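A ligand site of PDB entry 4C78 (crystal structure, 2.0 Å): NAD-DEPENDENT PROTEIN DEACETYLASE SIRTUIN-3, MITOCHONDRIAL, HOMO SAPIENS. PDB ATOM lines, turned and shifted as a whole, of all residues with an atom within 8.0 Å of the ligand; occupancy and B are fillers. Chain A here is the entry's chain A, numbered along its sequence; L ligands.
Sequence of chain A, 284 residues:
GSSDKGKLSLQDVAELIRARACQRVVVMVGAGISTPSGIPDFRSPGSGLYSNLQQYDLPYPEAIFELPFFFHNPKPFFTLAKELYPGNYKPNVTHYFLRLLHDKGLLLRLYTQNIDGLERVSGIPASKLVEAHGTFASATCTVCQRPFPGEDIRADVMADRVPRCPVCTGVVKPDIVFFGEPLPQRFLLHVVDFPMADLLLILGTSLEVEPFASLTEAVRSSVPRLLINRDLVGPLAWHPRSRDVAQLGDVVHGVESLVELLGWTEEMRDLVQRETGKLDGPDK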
ATOM      1  N   ALA A  21     -12.539  18.161  18.800  1.00  0.00           N
ATOM      2  CA  ALA A  21     -13.464  17.702  19.835  1.00  0.00           C
ATOM      3  C   ALA A  21     -13.897  16.238  19.571  1.00  0.00           C
ATOM      4  O   ALA A  21     -14.383  15.576  20.486  1.00  0.00           O
ATOM      5  CB  ALA A  21     -14.691  18.581  19.823  1.00  0.00           C
ATOM      6  N   CYS A  22     -13.730  15.741  18.339  1.00  0.00           N
ATOM      7  CA  CYS A  22     -13.986  14.352  18.017  1.00  0.00           C
ATOM      8  C   CYS A  22     -12.652  13.605  17.935  1.00  0.00           C
ATOM      9  O   CYS A  22     -11.923  13.591  16.910  1.00  0.00           O
ATOM     10  CB  CYS A  22     -14.819  14.266  16.730  1.00  0.00           C
ATOM     11  SG  CYS A  22     -16.593  14.515  17.009  1.00  0.00           S
ATOM     12  N   GLN A  23     -12.285  12.954  19.003  1.00  0.00           N
ATOM     13  CA  GLN A  23     -10.935  12.409  19.064  1.00  0.00           C
ATOM     14  C   GLN A  23     -10.924  10.981  19.011  1.00  0.00           C
ATOM     15  O   GLN A  23      -9.867  10.383  19.186  1.00  0.00           O
ATOM     16  CB  GLN A  23     -10.265  12.822  20.366  1.00  0.00           C
ATOM     17  CG  GLN A  23      -9.205  13.877  20.144  1.00  0.00           C
ATOM     18  CD  GLN A  23      -9.092  14.656  21.383  1.00  0.00           C
ATOM     19  OE1 GLN A  23      -9.278  14.123  22.469  1.00  0.00           O
ATOM     20  NE2 GLN A  23      -8.896  15.934  21.254  1.00  0.00           N
ATOM     21  N   ARG A  24     -12.129  10.397  18.846  1.00  0.00           N
ATOM     22  CA  ARG A  24     -12.288   8.966  18.956  1.00  0.00           C
ATOM     23  C   ARG A  24     -13.314   8.538  17.928  1.00  0.00           C
ATOM     24  O   ARG A  24     -14.392   8.067  18.282  1.00  0.00           O
ATOM     25  CB  ARG A  24     -12.737   8.539  20.323  1.00  0.00           C
ATOM     26  CG  ARG A  24     -11.599   8.144  21.256  1.00  0.00           C
ATOM     27  CD  ARG A  24     -12.164   7.948  22.676  1.00  0.00           C
ATOM     28  NE  ARG A  24     -12.165   9.311  23.178  1.00  0.00           N
ATOM     29  CZ  ARG A  24     -11.309   9.799  24.069  1.00  0.00           C
ATOM     30  NH1 ARG A  24     -10.454   9.020  24.725  1.00  0.00           N
ATOM     31  NH2 ARG A  24     -11.389  11.081  24.326  1.00  0.00           N
ATOM     32  N   VAL A  25     -12.949   8.741  16.676  1.00  0.00           N
ATOM     33  CA  VAL A  25     -13.764   8.411  15.532  1.00  0.00           C
ATOM     34  C   VAL A  25     -13.672   6.962  15.242  1.00  0.00           C
ATOM     35  O   VAL A  25     -12.607   6.409  15.202  1.00  0.00           O
ATOM     36  CB  VAL A  25     -13.371   9.214  14.278  1.00  0.00           C
ATOM     37  CG1 VAL A  25     -14.384   8.979  13.188  1.00  0.00           C
ATOM     38  CG2 VAL A  25     -13.370  10.695  14.666  1.00  0.00           C
ATOM     39  N   LEU A 108     -10.085   6.096  16.329  1.00  0.00           N
ATOM     40  CA  LEU A 108     -10.104   5.027  17.328  1.00  0.00           C
ATOM     41  C   LEU A 108      -9.973   3.683  16.599  1.00  0.00           C
ATOM     42  O   LEU A 108      -9.137   2.888  16.941  1.00  0.00           O
ATOM     43  CB  LEU A 108     -11.350   5.118  18.158  1.00  0.00           C
ATOM     44  CG  LEU A 108     -11.639   3.974  19.137  1.00  0.00           C
ATOM     45  CD1 LEU A 108     -10.407   3.650  19.950  1.00  0.00           C
ATOM     46  CD2 LEU A 108     -12.800   4.368  19.980  1.00  0.00           C
ATOM     47  N   VAL A 192     -16.433  -2.750  22.831  1.00  0.00           N
ATOM     48  CA  VAL A 192     -16.178  -1.501  23.504  1.00  0.00           C
ATOM     49  C   VAL A 192     -15.818  -0.336  22.556  1.00  0.00           C
ATOM     50  O   VAL A 192     -16.040   0.792  22.943  1.00  0.00           O
ATOM     51  CB  VAL A 192     -15.104  -1.633  24.574  1.00  0.00           C
ATOM     52  CG1 VAL A 192     -15.589  -2.589  25.642  1.00  0.00           C
ATOM     53  CG2 VAL A 192     -13.819  -2.107  23.981  1.00  0.00           C
ATOM     54  N   ASP A 193     -15.293  -0.583  21.345  1.00  0.00           N
ATOM     55  CA  ASP A 193     -15.067   0.553  20.418  1.00  0.00           C
ATOM     56  C   ASP A 193     -16.293   1.381  20.187  1.00  0.00           C
ATOM     57  O   ASP A 193     -16.222   2.598  20.183  1.00  0.00           O
ATOM     58  CB  ASP A 193     -14.449   0.150  19.051  1.00  0.00           C
ATOM     59  CG  ASP A 193     -12.994  -0.411  19.154  1.00  0.00           C
ATOM     60  OD1 ASP A 193     -12.270  -0.157  20.173  1.00  0.00           O
ATOM     61  OD2 ASP A 193     -12.567  -1.061  18.125  1.00  0.00           O
ATOM     62  N   PHE A 194     -17.458   0.767  20.038  1.00  0.00           N
ATOM     63  CA  PHE A 194     -18.600   1.579  19.674  1.00  0.00           C
ATOM     64  C   PHE A 194     -19.130   2.550  20.759  1.00  0.00           C
ATOM     65  O   PHE A 194     -19.322   3.705  20.476  1.00  0.00           O
ATOM     66  CB  PHE A 194     -19.654   0.728  18.989  1.00  0.00           C
ATOM     67  CG  PHE A 194     -19.251   0.367  17.551  1.00  0.00           C
ATOM     68  CD1 PHE A 194     -18.323  -0.582  17.324  1.00  0.00           C
ATOM     69  CD2 PHE A 194     -19.763   1.081  16.467  1.00  0.00           C
ATOM     70  CE1 PHE A 194     -17.909  -0.881  16.002  1.00  0.00           C
ATOM     71  CE2 PHE A 194     -19.365   0.810  15.193  1.00  0.00           C
ATOM     72  CZ  PHE A 194     -18.411  -0.156  14.958  1.00  0.00           C
ATOM     73  N   PRO A 195     -19.287   2.071  22.019  1.00  0.00           N
ATOM     74  CA  PRO A 195     -19.603   2.982  23.134  1.00  0.00           C
ATOM     75  C   PRO A 195     -18.482   3.986  23.428  1.00  0.00           C
ATOM     76  O   PRO A 195     -18.746   5.056  23.960  1.00  0.00           O
ATOM     77  CB  PRO A 195     -19.830   2.048  24.343  1.00  0.00           C
ATOM     78  CG  PRO A 195     -19.442   0.686  23.930  1.00  0.00           C
ATOM     79  CD  PRO A 195     -19.162   0.681  22.431  1.00  0.00           C
ATOM     80  N   MET A 196     -17.241   3.650  23.069  1.00  0.00           N
ATOM     81  CA  MET A 196     -16.097   4.542  23.253  1.00  0.00           C
ATOM     82  C   MET A 196     -15.981   5.673  22.231  1.00  0.00           C
ATOM     83  O   MET A 196     -15.287   6.663  22.462  1.00  0.00           O
ATOM     84  CB  MET A 196     -14.772   3.774  23.305  1.00  0.00           C
ATOM     85  CG  MET A 196     -14.585   2.853  24.550  1.00  0.00           C
ATOM     86  SD  MET A 196     -14.381   3.848  26.086  1.00  0.00           S
ATOM     87  CE  MET A 196     -16.107   4.119  26.356  1.00  0.00           C
ATOM     88  N   ALA A 197     -16.710   5.543  21.120  1.00  0.00           N
ATOM     89  CA  ALA A 197     -16.608   6.537  20.056  1.00  0.00           C
ATOM     90  C   ALA A 197     -17.228   7.806  20.468  1.00  0.00           C
ATOM     91  O   ALA A 197     -18.242   7.838  21.189  1.00  0.00           O
ATOM     92  CB  ALA A 197     -17.304   6.021  18.787  1.00  0.00           C
ATOM     93  N   ASP A 198     -16.669   8.892  19.962  1.00  0.00           N
ATOM     94  CA  ASP A 198     -17.351  10.202  20.033  1.00  0.00           C
ATOM     95  C   ASP A 198     -17.833  10.683  18.632  1.00  0.00           C
ATOM     96  O   ASP A 198     -18.456  11.781  18.470  1.00  0.00           O
ATOM     97  CB  ASP A 198     -16.505  11.227  20.753  1.00  0.00           C
ATOM     98  CG  ASP A 198     -15.150  11.532  20.078  1.00  0.00           C
ATOM     99  OD1 ASP A 198     -14.811  11.140  18.909  1.00  0.00           O
ATOM    100  OD2 ASP A 198     -14.351  12.191  20.787  1.00  0.00           O
ATOM    101  N   LEU A 199     -17.641   9.818  17.657  1.00  0.00           N
ATOM    102  CA  LEU A 199     -18.135  10.004  16.315  1.00  0.00           C
ATOM    103  C   LEU A 199     -18.118   8.697  15.592  1.00  0.00           C
ATOM    104  O   LEU A 199     -17.144   7.943  15.662  1.00  0.00           O
ATOM    105  CB  LEU A 199     -17.267  10.930  15.502  1.00  0.00           C
ATOM    106  CG  LEU A 199     -17.772  11.252  14.081  1.00  0.00           C
ATOM    107  CD1 LEU A 199     -19.115  11.869  14.148  1.00  0.00           C
ATOM    108  CD2 LEU A 199     -16.818  12.186  13.324  1.00  0.00           C
ATOM    109  N   ARG A 220     -23.220   5.717  21.614  1.00  0.00           N
ATOM    110  CA  ARG A 220     -23.999   6.335  22.667  1.00  0.00           C
ATOM    111  C   ARG A 220     -24.908   7.338  21.994  1.00  0.00           C
ATOM    112  O   ARG A 220     -24.665   7.813  20.874  1.00  0.00           O
ATOM    113  CB  ARG A 220     -23.119   7.020  23.725  1.00  0.00           C
ATOM    114  CG  ARG A 220     -22.108   6.100  24.362  1.00  0.00           C
ATOM    115  CD  ARG A 220     -21.096   6.792  25.255  1.00  0.00           C
ATOM    116  NE  ARG A 220     -20.148   7.478  24.408  1.00  0.00           N
ATOM    117  CZ  ARG A 220     -19.941   8.771  24.400  1.00  0.00           C
ATOM    118  NH1 ARG A 220     -20.550   9.558  25.282  1.00  0.00           N
ATOM    119  NH2 ARG A 220     -19.081   9.283  23.550  1.00  0.00           N
ATOM    120  N   SER A 222     -25.820  10.478  22.251  1.00  0.00           N
ATOM    121  CA  SER A 222     -25.364  11.815  21.932  1.00  0.00           C
ATOM    122  C   SER A 222     -24.349  11.892  20.792  1.00  0.00           C
ATOM    123  O   SER A 222     -23.988  12.970  20.360  1.00  0.00           O
ATOM    124  CB  SER A 222     -24.635  12.307  23.170  1.00  0.00           C
ATOM    125  OG  SER A 222     -23.535  11.429  23.418  1.00  0.00           O
ATOM    126  N   VAL A 223     -23.873  10.746  20.341  1.00  0.00           N
ATOM    127  CA  VAL A 223     -22.817  10.679  19.388  1.00  0.00           C
ATOM    128  C   VAL A 223     -23.376  10.821  17.997  1.00  0.00           C
ATOM    129  O   VAL A 223     -24.328  10.091  17.579  1.00  0.00           O
ATOM    130  CB  VAL A 223     -21.973   9.395  19.583  1.00  0.00           C
ATOM    131  CG1 VAL A 223     -20.957   9.219  18.511  1.00  0.00           C
ATOM    132  CG2 VAL A 223     -21.211   9.491  20.905  1.00  0.00           C
HETATM  133  O1  LIG L   1     -15.062   8.991  23.272  1.00  0.00           O
HETATM  134  O2  LIG L   1     -16.128  12.223  26.652  1.00  0.00           O
HETATM  135 BR1  LIG L   1     -21.596   2.878  30.427  1.00  0.00          BR
HETATM  136  C1  LIG L   1     -17.487   6.538  27.391  1.00  0.00           C
HETATM  137  C2  LIG L   1     -17.893   7.915  27.012  1.00  0.00           C
HETATM  138  C3  LIG L   1     -19.141   3.468  28.838  1.00  0.00           C
HETATM  139  C4  LIG L   1     -20.445   5.358  29.445  1.00  0.00           C
HETATM  140  C5  LIG L   1     -18.242   4.283  28.153  1.00  0.00           C
HETATM  141  C6  LIG L   1     -19.531   6.191  28.761  1.00  0.00           C
HETATM  142  C7  LIG L   1     -15.502  10.680  24.930  1.00  0.00           C
HETATM  143  C8  LIG L   1     -16.417   8.408  25.141  1.00  0.00           C
HETATM  144  C9  LIG L   1     -16.960  10.057  26.795  1.00  0.00           C
HETATM  145  C10 LIG L   1     -15.678   9.374  24.420  1.00  0.00           C
HETATM  146  C11 LIG L   1     -16.183  11.006  26.093  1.00  0.00           C
HETATM  147  C12 LIG L   1     -20.257   4.012  29.482  1.00  0.00           C
HETATM  148  C13 LIG L   1     -18.430   5.690  28.094  1.00  0.00           C
HETATM  149  C14 LIG L   1     -17.070   8.781  26.307  1.00  0.00           C
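The backbone NH of Arg 24 sits at hydrogen-bond distance from the side-chain carboxylate of Asp 198, at 2.8 Å. O of Ala 197 sits at hydrogen-bond distance from NH2 of Arg 220, 2.9 Å away. The guanidinium group of Arg 220 sits at hydrogen-bond distance from the backbone carbonyl oxygen of Pro 195. OD2 of Asp 198 is in hydrogen-bond range of N of Gln 23 (2.8 Å). The side-chain sulfur (SG) of Cys 22 lies within hydrogen-bond range of the backbone carbonyl oxygen (O) of Asp 198.
Pro 195 touches the ligand. Ala 197 touches the ligand (C to O1, 3.7 Å). CB of Asp 198 touches O1 of the ligand, 3.7 Å away. NH2 of Arg 220 touches C8 of the ligand, 3.2 Å away. Hydrophobic or aromatic side chains within 4 Å of the ligand: Met 196. Within 4 Å of the ligand: Arg 24, Pro 195, Met 196, Ala 197, Asp 198 and Arg 220. The nearest printed residue that does not touch the ligand is Leu 108 (6.1 Å).
O of Met 196 lies within hydrogen-bond range of O1 of the ligand (2.5 Å). NE of Arg 24 sits at hydrogen-bond distance from O1 of the ligand, at 2.9 Å.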
